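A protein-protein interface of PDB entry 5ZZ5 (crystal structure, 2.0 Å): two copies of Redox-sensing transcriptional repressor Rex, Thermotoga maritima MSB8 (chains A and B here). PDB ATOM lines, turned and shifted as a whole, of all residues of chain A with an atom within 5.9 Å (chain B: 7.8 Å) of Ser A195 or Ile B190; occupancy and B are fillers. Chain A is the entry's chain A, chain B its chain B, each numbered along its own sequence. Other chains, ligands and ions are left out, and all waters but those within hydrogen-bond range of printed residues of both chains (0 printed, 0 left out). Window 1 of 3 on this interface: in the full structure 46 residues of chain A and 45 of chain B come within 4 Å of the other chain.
Printed residues of chain B that touch a printed residue of chain A: Phe B108, Ile B148, Ile B173, Leu B174, Glu B188, Ile B190, Ile B192 and Ser B195.
Hydrophobic or aromatic side chains of chain B within 4 Å of the printed part of chain A: Phe B108, Ile B148, Leu B174 and Ile B190.
Of the 11 printed residues of chain A, 9 touch a printed residue of chain B.
Hydrophobic or aromatic side chains of chain A that line the printed part of chain B: Ile A190, Ile A192, Leu A196, Val A198 and Leu A199.
Among the printed residues, no Asp or Glu carboxylate lies within 4 Å of a Lys or Arg side-chain nitrogen of the other chain.
Ile A190 touches its own counterpart, Ile B190.
Ile A190 touches Ile B192, and with the chains exchanged Ile A192 touches Ile B190.
Ile A190 touches Ser B195, and with the chains exchanged Ser A195 touches Ile B190.
Positions printed for both chains: 190, 191, 192, 193, 194 and 195.
Ile B190 touches Ile A190 (CG2 to CG2, 3.7 Å).
CA of Ile B192 touches CD1 of Ile A190 (3.9 Å).
Ile A190 touches Ser B195.
CA of Ile A192 touches CD1 of Ile B190, 3.97 Å away.
Leu A196 touches Leu B174.
CE2 of Phe B108 touches NH2 of Arg A197, 3.4 Å away.
Leu A199 touches Ile B148 (CD2 to CG2, 3.98 Å).
Leu A199 touches Ile B173.
CD2 of Leu A199 touches N of Leu B174, 3.9 Å away.
Glu B188 touches Leu A199 (CG to CB, 3.8 Å).
Of the printed residues of chain B, Thr A193 touches Phe B108.
No residue of chain B comes within 4 Å of Ala A194.
Of chain B, only Glu B188 and Ile B190 come within 4 Å of Ser A195.
Of the printed residues of chain A, Phe B108 touches Thr A193 (3.9 Å), Leu A196 (3.7 Å), Arg A197 (3.4 Å) and Thr A200 (3.6 Å).
Ile B151 touches none of the printed residues of chain A.
Of the printed residues of chain A, Ile B173 touches Leu A199 (3.6 Å).
Ile B190 touches three residues of chain A.
Ala B194 touches none of the printed residues of chain A.
Of the printed residues of chain A, Ser B195 touches Ile A190.
The nearest printed residue of chain B that does not touch Leu A196 is Ile B148 (4.1 Å).
The backbone NH (N) of Thr A193 sits close to the side-chain carboxylate (OD1) of Asp A191 (3.3 Å).
N of Glu B188 sits at hydrogen-bond distance from O of Ile B173.
O of Asp B191 sits at hydrogen-bond distance from OG of Ser B195 (3.5 Å).
The backbone carbonyl oxygen (O) of Leu B174 is in hydrogen-bond range of the backbone NH (N) of Ile B151 (2.9 Å).
The backbone carbonyl oxygen of Asp A191 lies within hydrogen-bond range of the side-chain hydroxyl of Ser A195 (3.5 Å).
The backbone carbonyl oxygen of Glu B188 lies within hydrogen-bond range of the backbone NH of Asn B175 (2.7 Å).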
ATOM      1  N   ILE A 190      -4.809  -6.090  -3.181  1.00  0.00           N
ATOM      2  CA  ILE A 190      -4.030  -4.936  -3.626  1.00  0.00           C
ATOM      3  C   ILE A 190      -4.741  -4.478  -4.872  1.00  0.00           C
ATOM      4  O   ILE A 190      -4.853  -5.219  -5.857  1.00  0.00           O
ATOM      5  CB  ILE A 190      -2.556  -5.276  -3.900  1.00  0.00           C
ATOM      6  CG1 ILE A 190      -1.868  -5.738  -2.614  1.00  0.00           C
ATOM      7  CG2 ILE A 190      -1.813  -4.082  -4.513  1.00  0.00           C
ATOM      8  CD1 ILE A 190      -0.377  -6.073  -2.788  1.00  0.00           C
ATOM      9  N   ASP A 191      -5.215  -3.246  -4.845  1.00  0.00           N
ATOM     10  CA  ASP A 191      -5.997  -2.719  -5.961  1.00  0.00           C
ATOM     11  C   ASP A 191      -5.430  -1.339  -6.190  1.00  0.00           C
ATOM     12  O   ASP A 191      -5.763  -0.392  -5.466  1.00  0.00           O
ATOM     13  CB  ASP A 191      -7.498  -2.672  -5.613  1.00  0.00           C
ATOM     14  CG  ASP A 191      -8.365  -2.203  -6.770  1.00  0.00           C
ATOM     15  OD1 ASP A 191      -7.853  -1.551  -7.700  1.00  0.00           O
ATOM     16  OD2 ASP A 191      -9.573  -2.473  -6.750  1.00  0.00           O
ATOM     17  N   ILE A 192      -4.567  -1.243  -7.198  1.00  0.00           N
ATOM     18  CA  ILE A 192      -3.805  -0.035  -7.479  1.00  0.00           C
ATOM     19  C   ILE A 192      -4.752   1.133  -7.727  1.00  0.00           C
ATOM     20  O   ILE A 192      -4.582   2.219  -7.188  1.00  0.00           O
ATOM     21  CB  ILE A 192      -2.885  -0.250  -8.704  1.00  0.00           C
ATOM     22  CG1 ILE A 192      -1.805  -1.300  -8.371  1.00  0.00           C
ATOM     23  CG2 ILE A 192      -2.259   1.067  -9.149  1.00  0.00           C
ATOM     24  CD1 ILE A 192      -1.067  -1.886  -9.615  1.00  0.00           C
ATOM     25  N   THR A 193      -5.798   0.860  -8.487  1.00  0.00           N
ATOM     26  CA  THR A 193      -6.824   1.858  -8.764  1.00  0.00           C
ATOM     27  C   THR A 193      -7.575   2.317  -7.508  1.00  0.00           C
ATOM     28  O   THR A 193      -7.842   3.515  -7.352  1.00  0.00           O
ATOM     29  CB  THR A 193      -7.801   1.317  -9.804  1.00  0.00           C
ATOM     30  OG1 THR A 193      -7.043   0.897 -10.943  1.00  0.00           O
ATOM     31  CG2 THR A 193      -8.766   2.401 -10.247  1.00  0.00           C
ATOM     32  N   ALA A 194      -7.939   1.384  -6.622  1.00  0.00           N
ATOM     33  CA  ALA A 194      -8.584   1.750  -5.366  1.00  0.00           C
ATOM     34  C   ALA A 194      -7.659   2.593  -4.477  1.00  0.00           C
ATOM     35  O   ALA A 194      -8.113   3.546  -3.845  1.00  0.00           O
ATOM     36  CB  ALA A 194      -9.053   0.488  -4.594  1.00  0.00           C
ATOM     37  N   SER A 195      -6.374   2.234  -4.408  1.00  0.00           N
ATOM     38  CA  SER A 195      -5.426   3.000  -3.597  1.00  0.00           C
ATOM     39  C   SER A 195      -5.319   4.424  -4.158  1.00  0.00           C
ATOM     40  O   SER A 195      -5.265   5.390  -3.399  1.00  0.00           O
ATOM     41  CB  SER A 195      -4.026   2.356  -3.576  1.00  0.00           C
ATOM     42  OG  SER A 195      -4.014   1.128  -2.882  1.00  0.00           O
ATOM     43  N   LEU A 196      -5.290   4.537  -5.483  1.00  0.00           N
ATOM     44  CA  LEU A 196      -5.251   5.848  -6.137  1.00  0.00           C
ATOM     45  C   LEU A 196      -6.504   6.653  -5.800  1.00  0.00           C
ATOM     46  O   LEU A 196      -6.435   7.859  -5.538  1.00  0.00           O
ATOM     47  CB  LEU A 196      -5.138   5.693  -7.648  1.00  0.00           C
ATOM     48  CG  LEU A 196      -3.727   5.313  -8.113  1.00  0.00           C
ATOM     49  CD1 LEU A 196      -3.729   4.859  -9.533  1.00  0.00           C
ATOM     50  CD2 LEU A 196      -2.755   6.483  -7.906  1.00  0.00           C
ATOM     51  N   ARG A 197      -7.642   5.971  -5.777  1.00  0.00           N
ATOM     52  CA  ARG A 197      -8.921   6.611  -5.466  1.00  0.00           C
ATOM     53  C   ARG A 197      -8.929   7.141  -4.036  1.00  0.00           C
ATOM     54  O   ARG A 197      -9.305   8.293  -3.793  1.00  0.00           O
ATOM     55  CB  ARG A 197     -10.074   5.630  -5.674  1.00  0.00           C
ATOM     56  CG  ARG A 197     -11.474   6.273  -5.644  1.00  0.00           C
ATOM     57  CD  ARG A 197     -11.626   7.396  -6.698  1.00  0.00           C
ATOM     58  NE  ARG A 197     -11.691   6.872  -8.050  1.00  0.00           N
ATOM     59  CZ  ARG A 197     -11.506   7.583  -9.157  1.00  0.00           C
ATOM     60  NH1 ARG A 197     -11.217   8.881  -9.101  1.00  0.00           N
ATOM     61  NH2 ARG A 197     -11.594   6.983 -10.330  1.00  0.00           N
ATOM     62  N   VAL A 198      -8.435   6.338  -3.100  1.00  0.00           N
ATOM     63  CA  VAL A 198      -8.306   6.779  -1.710  1.00  0.00           C
ATOM     64  C   VAL A 198      -7.422   8.021  -1.618  1.00  0.00           C
ATOM     65  O   VAL A 198      -7.757   8.980  -0.925  1.00  0.00           O
ATOM     66  CB  VAL A 198      -7.756   5.645  -0.796  1.00  0.00           C
ATOM     67  CG1 VAL A 198      -7.249   6.198   0.503  1.00  0.00           C
ATOM     68  CG2 VAL A 198      -8.850   4.576  -0.558  1.00  0.00           C
ATOM     69  N   LEU A 199      -6.299   7.995  -2.331  1.00  0.00           N
ATOM     70  CA  LEU A 199      -5.388   9.135  -2.380  1.00  0.00           C
ATOM     71  C   LEU A 199      -6.108  10.385  -2.923  1.00  0.00           C
ATOM     72  O   LEU A 199      -5.997  11.464  -2.342  1.00  0.00           O
ATOM     73  CB  LEU A 199      -4.162   8.798  -3.244  1.00  0.00           C
ATOM     74  CG  LEU A 199      -3.098   9.878  -3.421  1.00  0.00           C
ATOM     75  CD1 LEU A 199      -2.480  10.247  -2.100  1.00  0.00           C
ATOM     76  CD2 LEU A 199      -2.032   9.384  -4.431  1.00  0.00           C
ATOM     77  N   THR A 200      -6.847  10.251  -4.024  1.00  0.00           N
ATOM     78  CA  THR A 200      -7.524  11.420  -4.596  1.00  0.00           C
ATOM     79  C   THR A 200      -8.560  11.995  -3.620  1.00  0.00           C
ATOM     80  O   THR A 200      -8.752  13.207  -3.583  1.00  0.00           O
ATOM     81  CB  THR A 200      -8.238  11.119  -5.930  1.00  0.00           C
ATOM     82  OG1 THR A 200      -9.177  10.055  -5.774  1.00  0.00           O
ATOM     83  CG2 THR A 200      -7.222  10.777  -7.020  1.00  0.00           C
ATOM     84  N   ILE B  93       8.322  -2.600 -11.564  1.00  0.00           N
ATOM     85  CA  ILE B  93       7.101  -2.005 -11.057  1.00  0.00           C
ATOM     86  C   ILE B  93       6.607  -0.814 -11.880  1.00  0.00           C
ATOM     87  O   ILE B  93       5.417  -0.736 -12.222  1.00  0.00           O
ATOM     88  CB  ILE B  93       7.317  -1.567  -9.611  1.00  0.00           C
ATOM     89  CG1 ILE B  93       7.550  -2.816  -8.745  1.00  0.00           C
ATOM     90  CG2 ILE B  93       6.157  -0.722  -9.154  1.00  0.00           C
ATOM     91  CD1 ILE B  93       8.104  -2.537  -7.348  1.00  0.00           C
ATOM     92  N   VAL B  97       3.059  -0.583 -13.834  1.00  0.00           N
ATOM     93  CA  VAL B  97       2.068   0.466 -13.588  1.00  0.00           C
ATOM     94  C   VAL B  97       1.761   1.222 -14.872  1.00  0.00           C
ATOM     95  O   VAL B  97       0.596   1.537 -15.130  1.00  0.00           O
ATOM     96  CB  VAL B  97       2.510   1.453 -12.453  1.00  0.00           C
ATOM     97  CG1 VAL B  97       1.531   2.649 -12.328  1.00  0.00           C
ATOM     98  CG2 VAL B  97       2.608   0.715 -11.106  1.00  0.00           C
ATOM     99  N   PHE B 108      -7.457   7.424 -14.352  1.00  0.00           N
ATOM    100  CA  PHE B 108      -6.091   7.729 -13.962  1.00  0.00           C
ATOM    101  C   PHE B 108      -5.146   7.646 -15.160  1.00  0.00           C
ATOM    102  O   PHE B 108      -4.884   6.571 -15.676  1.00  0.00           O
ATOM    103  CB  PHE B 108      -5.653   6.805 -12.844  1.00  0.00           C
ATOM    104  CG  PHE B 108      -6.469   6.970 -11.580  1.00  0.00           C
ATOM    105  CD1 PHE B 108      -6.220   8.037 -10.724  1.00  0.00           C
ATOM    106  CD2 PHE B 108      -7.506   6.099 -11.287  1.00  0.00           C
ATOM    107  CE1 PHE B 108      -6.962   8.214  -9.569  1.00  0.00           C
ATOM    108  CE2 PHE B 108      -8.256   6.264 -10.111  1.00  0.00           C
ATOM    109  CZ  PHE B 108      -7.983   7.323  -9.261  1.00  0.00           C
ATOM    110  N   ILE B 148      -0.546  13.563  -9.444  1.00  0.00           N
ATOM    111  CA  ILE B 148      -0.109  12.399  -8.682  1.00  0.00           C
ATOM    112  C   ILE B 148       1.222  11.874  -9.208  1.00  0.00           C
ATOM    113  O   ILE B 148       1.419  11.725 -10.420  1.00  0.00           O
ATOM    114  CB  ILE B 148      -1.192  11.297  -8.717  1.00  0.00           C
ATOM    115  CG1 ILE B 148      -2.450  11.776  -7.953  1.00  0.00           C
ATOM    116  CG2 ILE B 148      -0.670   9.972  -8.124  1.00  0.00           C
ATOM    117  CD1 ILE B 148      -3.691  10.893  -8.200  1.00  0.00           C
ATOM    118  N   ILE B 151       5.889   6.616  -7.147  1.00  0.00           N
ATOM    119  CA  ILE B 151       7.285   6.369  -6.887  1.00  0.00           C
ATOM    120  C   ILE B 151       7.580   4.897  -7.018  1.00  0.00           C
ATOM    121  O   ILE B 151       7.076   4.091  -6.231  1.00  0.00           O
ATOM    122  CB  ILE B 151       7.702   6.870  -5.495  1.00  0.00           C
ATOM    123  CG1 ILE B 151       7.577   8.386  -5.436  1.00  0.00           C
ATOM    124  CG2 ILE B 151       9.144   6.470  -5.198  1.00  0.00           C
ATOM    125  CD1 ILE B 151       8.070   8.963  -4.147  1.00  0.00           C
ATOM    126  N   ILE B 173       1.079  11.320  -3.620  1.00  0.00           N
ATOM    127  CA  ILE B 173       2.043  10.322  -4.045  1.00  0.00           C
ATOM    128  C   ILE B 173       1.532   8.911  -3.765  1.00  0.00           C
ATOM    129  O   ILE B 173       1.030   8.641  -2.684  1.00  0.00           O
ATOM    130  CB  ILE B 173       3.377  10.536  -3.336  1.00  0.00           C
ATOM    131  CG1 ILE B 173       4.057  11.802  -3.907  1.00  0.00           C
ATOM    132  CG2 ILE B 173       4.286   9.298  -3.493  1.00  0.00           C
ATOM    133  CD1 ILE B 173       5.297  12.253  -3.128  1.00  0.00           C
ATOM    134  N   LEU B 174       1.620   8.049  -4.772  1.00  0.00           N
ATOM    135  CA  LEU B 174       1.446   6.608  -4.617  1.00  0.00           C
ATOM    136  C   LEU B 174       2.838   5.998  -4.547  1.00  0.00           C
ATOM    137  O   LEU B 174       3.616   6.064  -5.512  1.00  0.00           O
ATOM    138  CB  LEU B 174       0.652   6.002  -5.785  1.00  0.00           C
ATOM    139  CG  LEU B 174       0.469   4.490  -5.672  1.00  0.00           C
ATOM    140  CD1 LEU B 174      -0.396   4.168  -4.445  1.00  0.00           C
ATOM    141  CD2 LEU B 174      -0.163   3.945  -6.902  1.00  0.00           C
ATOM    142  N   ASN B 175       3.159   5.401  -3.407  1.00  0.00           N
ATOM    143  CA  ASN B 175       4.516   4.952  -3.148  1.00  0.00           C
ATOM    144  C   ASN B 175       4.646   3.426  -3.119  1.00  0.00           C
ATOM    145  O   ASN B 175       4.028   2.753  -2.268  1.00  0.00           O
ATOM    146  CB  ASN B 175       5.018   5.536  -1.829  1.00  0.00           C
ATOM    147  CG  ASN B 175       6.395   4.995  -1.446  1.00  0.00           C
ATOM    148  OD1 ASN B 175       7.276   4.854  -2.289  1.00  0.00           O
ATOM    149  ND2 ASN B 175       6.560   4.641  -0.185  1.00  0.00           N
ATOM    150  N   PHE B 176       5.452   2.892  -4.047  1.00  0.00           N
ATOM    151  CA  PHE B 176       5.803   1.467  -4.093  1.00  0.00           C
ATOM    152  C   PHE B 176       7.162   1.156  -3.471  1.00  0.00           C
ATOM    153  O   PHE B 176       7.539  -0.010  -3.380  1.00  0.00           O
ATOM    154  CB  PHE B 176       5.847   0.950  -5.527  1.00  0.00           C
ATOM    155  CG  PHE B 176       4.522   0.797  -6.159  1.00  0.00           C
ATOM    156  CD1 PHE B 176       3.808  -0.381  -6.037  1.00  0.00           C
ATOM    157  CD2 PHE B 176       3.983   1.829  -6.897  1.00  0.00           C
ATOM    158  CE1 PHE B 176       2.587  -0.527  -6.651  1.00  0.00           C
ATOM    159  CE2 PHE B 176       2.751   1.681  -7.520  1.00  0.00           C
ATOM    160  CZ  PHE B 176       2.056   0.504  -7.387  1.00  0.00           C
ATOM    161  N   ALA B 177       7.921   2.173  -3.077  1.00  0.00           N
ATOM    162  CA  ALA B 177       9.233   1.890  -2.480  1.00  0.00           C
ATOM    163  C   ALA B 177       9.044   1.441  -1.031  1.00  0.00           C
ATOM    164  O   ALA B 177       8.204   2.011  -0.317  1.00  0.00           O
ATOM    165  CB  ALA B 177      10.132   3.100  -2.536  1.00  0.00           C
ATOM    166  N   PRO B 178       9.816   0.423  -0.591  1.00  0.00           N
ATOM    167  CA  PRO B 178       9.731  -0.116   0.776  1.00  0.00           C
ATOM    168  C   PRO B 178      10.374   0.807   1.781  1.00  0.00           C
ATOM    169  O   PRO B 178      11.388   0.476   2.406  1.00  0.00           O
ATOM    170  CB  PRO B 178      10.502  -1.433   0.683  1.00  0.00           C
ATOM    171  CG  PRO B 178      11.524  -1.168  -0.393  1.00  0.00           C
ATOM    172  CD  PRO B 178      10.804  -0.309  -1.407  1.00  0.00           C
ATOM    173  N   VAL B 179       9.776   1.978   1.922  1.00  0.00           N
ATOM    174  CA  VAL B 179      10.249   2.982   2.857  1.00  0.00           C
ATOM    175  C   VAL B 179       9.083   3.926   3.100  1.00  0.00           C
ATOM    176  O   VAL B 179       8.200   4.052   2.258  1.00  0.00           O
ATOM    177  CB  VAL B 179      11.471   3.720   2.314  1.00  0.00           C
ATOM    178  CG1 VAL B 179      11.135   4.425   1.013  1.00  0.00           C
ATOM    179  CG2 VAL B 179      12.042   4.695   3.334  1.00  0.00           C
ATOM    180  N   LYS B 180       9.039   4.534   4.272  1.00  0.00           N
ATOM    181  CA  LYS B 180       8.007   5.508   4.561  1.00  0.00           C
ATOM    182  C   LYS B 180       8.543   6.862   4.176  1.00  0.00           C
ATOM    183  O   LYS B 180       9.562   7.303   4.698  1.00  0.00           O
ATOM    184  CB  LYS B 180       7.599   5.447   6.032  1.00  0.00           C
ATOM    185  CG  LYS B 180       6.884   4.146   6.385  1.00  0.00           C
ATOM    186  CD  LYS B 180       5.771   3.884   5.366  1.00  0.00           C
ATOM    187  CE  LYS B 180       5.351   2.430   5.341  1.00  0.00           C
ATOM    188  NZ  LYS B 180       6.476   1.529   4.982  1.00  0.00           N
ATOM    189  N   VAL B 187       0.234  10.540   1.129  1.00  0.00           N
ATOM    190  CA  VAL B 187       0.911   9.400   0.511  1.00  0.00           C
ATOM    191  C   VAL B 187       0.084   8.133   0.716  1.00  0.00           C
ATOM    192  O   VAL B 187      -0.418   7.904   1.816  1.00  0.00           O
ATOM    193  CB  VAL B 187       2.312   9.219   1.116  1.00  0.00           C
ATOM    194  CG1 VAL B 187       2.990   7.944   0.596  1.00  0.00           C
ATOM    195  CG2 VAL B 187       3.158  10.452   0.850  1.00  0.00           C
ATOM    196  N   GLU B 188      -0.087   7.334  -0.335  1.00  0.00           N
ATOM    197  CA  GLU B 188      -0.635   5.982  -0.194  1.00  0.00           C
ATOM    198  C   GLU B 188       0.470   5.020  -0.574  1.00  0.00           C
ATOM    199  O   GLU B 188       1.134   5.205  -1.595  1.00  0.00           O
ATOM    200  CB  GLU B 188      -1.843   5.727  -1.105  1.00  0.00           C
ATOM    201  CG  GLU B 188      -3.151   6.224  -0.602  1.00  0.00           C
ATOM    202  CD  GLU B 188      -3.603   5.541   0.685  1.00  0.00           C
ATOM    203  OE1 GLU B 188      -3.632   4.301   0.759  1.00  0.00           O
ATOM    204  OE2 GLU B 188      -3.934   6.289   1.590  1.00  0.00           O
ATOM    205  N   ASN B 189       0.717   4.034   0.273  1.00  0.00           N
ATOM    206  CA  ASN B 189       1.776   3.071  -0.002  1.00  0.00           C
ATOM    207  C   ASN B 189       1.207   1.770  -0.524  1.00  0.00           C
ATOM    208  O   ASN B 189       0.175   1.298  -0.041  1.00  0.00           O
ATOM    209  CB  ASN B 189       2.602   2.787   1.254  1.00  0.00           C
ATOM    210  CG  ASN B 189       3.143   4.044   1.894  1.00  0.00           C
ATOM    211  OD1 ASN B 189       3.975   4.744   1.320  1.00  0.00           O
ATOM    212  ND2 ASN B 189       2.681   4.332   3.101  1.00  0.00           N
ATOM    213  N   ILE B 190       1.879   1.175  -1.496  1.00  0.00           N
ATOM    214  CA  ILE B 190       1.598  -0.211  -1.842  1.00  0.00           C
ATOM    215  C   ILE B 190       2.873  -1.013  -1.628  1.00  0.00           C
ATOM    216  O   ILE B 190       3.961  -0.614  -2.068  1.00  0.00           O
ATOM    217  CB  ILE B 190       1.083  -0.355  -3.275  1.00  0.00           C
ATOM    218  CG1 ILE B 190      -0.289   0.314  -3.402  1.00  0.00           C
ATOM    219  CG2 ILE B 190       0.994  -1.836  -3.684  1.00  0.00           C
ATOM    220  CD1 ILE B 190      -0.898   0.175  -4.785  1.00  0.00           C
ATOM    221  N   ASP B 191       2.761  -2.076  -0.845  1.00  0.00           N
ATOM    222  CA  ASP B 191       3.915  -2.921  -0.537  1.00  0.00           C
ATOM    223  C   ASP B 191       3.458  -4.382  -0.495  1.00  0.00           C
ATOM    224  O   ASP B 191       2.766  -4.784   0.447  1.00  0.00           O
ATOM    225  CB  ASP B 191       4.544  -2.476   0.778  1.00  0.00           C
ATOM    226  CG  ASP B 191       5.818  -3.227   1.117  1.00  0.00           C
ATOM    227  OD1 ASP B 191       6.036  -4.342   0.611  1.00  0.00           O
ATOM    228  OD2 ASP B 191       6.620  -2.678   1.899  1.00  0.00           O
ATOM    229  N   ILE B 192       3.782  -5.153  -1.531  1.00  0.00           N
ATOM    230  CA  ILE B 192       3.266  -6.510  -1.608  1.00  0.00           C
ATOM    231  C   ILE B 192       3.742  -7.302  -0.390  1.00  0.00           C
ATOM    232  O   ILE B 192       2.990  -8.126   0.130  1.00  0.00           O
ATOM    233  CB  ILE B 192       3.640  -7.245  -2.908  1.00  0.00           C
ATOM    234  CG1 ILE B 192       2.866  -8.564  -2.991  1.00  0.00           C
ATOM    235  CG2 ILE B 192       5.098  -7.542  -2.964  1.00  0.00           C
ATOM    236  CD1 ILE B 192       3.165  -9.368  -4.194  1.00  0.00           C
ATOM    237  N   THR B 193       4.978  -7.055   0.064  1.00  0.00           N
ATOM    238  CA  THR B 193       5.479  -7.753   1.246  1.00  0.00           C
ATOM    239  C   THR B 193       4.660  -7.410   2.485  1.00  0.00           C
ATOM    240  O   THR B 193       4.328  -8.306   3.256  1.00  0.00           O
ATOM    241  CB  THR B 193       6.973  -7.444   1.540  1.00  0.00           C
ATOM    242  OG1 THR B 193       7.752  -7.681   0.365  1.00  0.00           O
ATOM    243  CG2 THR B 193       7.475  -8.345   2.642  1.00  0.00           C
ATOM    244  N   ALA B 194       4.317  -6.134   2.682  1.00  0.00           N
ATOM    245  CA  ALA B 194       3.461  -5.768   3.830  1.00  0.00           C
ATOM    246  C   ALA B 194       2.079  -6.449   3.741  1.00  0.00           C
ATOM    247  O   ALA B 194       1.519  -6.917   4.759  1.00  0.00           O
ATOM    248  CB  ALA B 194       3.289  -4.259   3.916  1.00  0.00           C
ATOM    249  N   SER B 195       1.521  -6.494   2.533  1.00  0.00           N
ATOM    250  CA  SER B 195       0.214  -7.120   2.341  1.00  0.00           C
ATOM    251  C   SER B 195       0.273  -8.602   2.665  1.00  0.00           C
ATOM    252  O   SER B 195      -0.646  -9.147   3.274  1.00  0.00           O
ATOM    253  CB  SER B 195      -0.301  -6.909   0.914  1.00  0.00           C
ATOM    254  OG  SER B 195      -0.597  -5.536   0.683  1.00  0.00           O
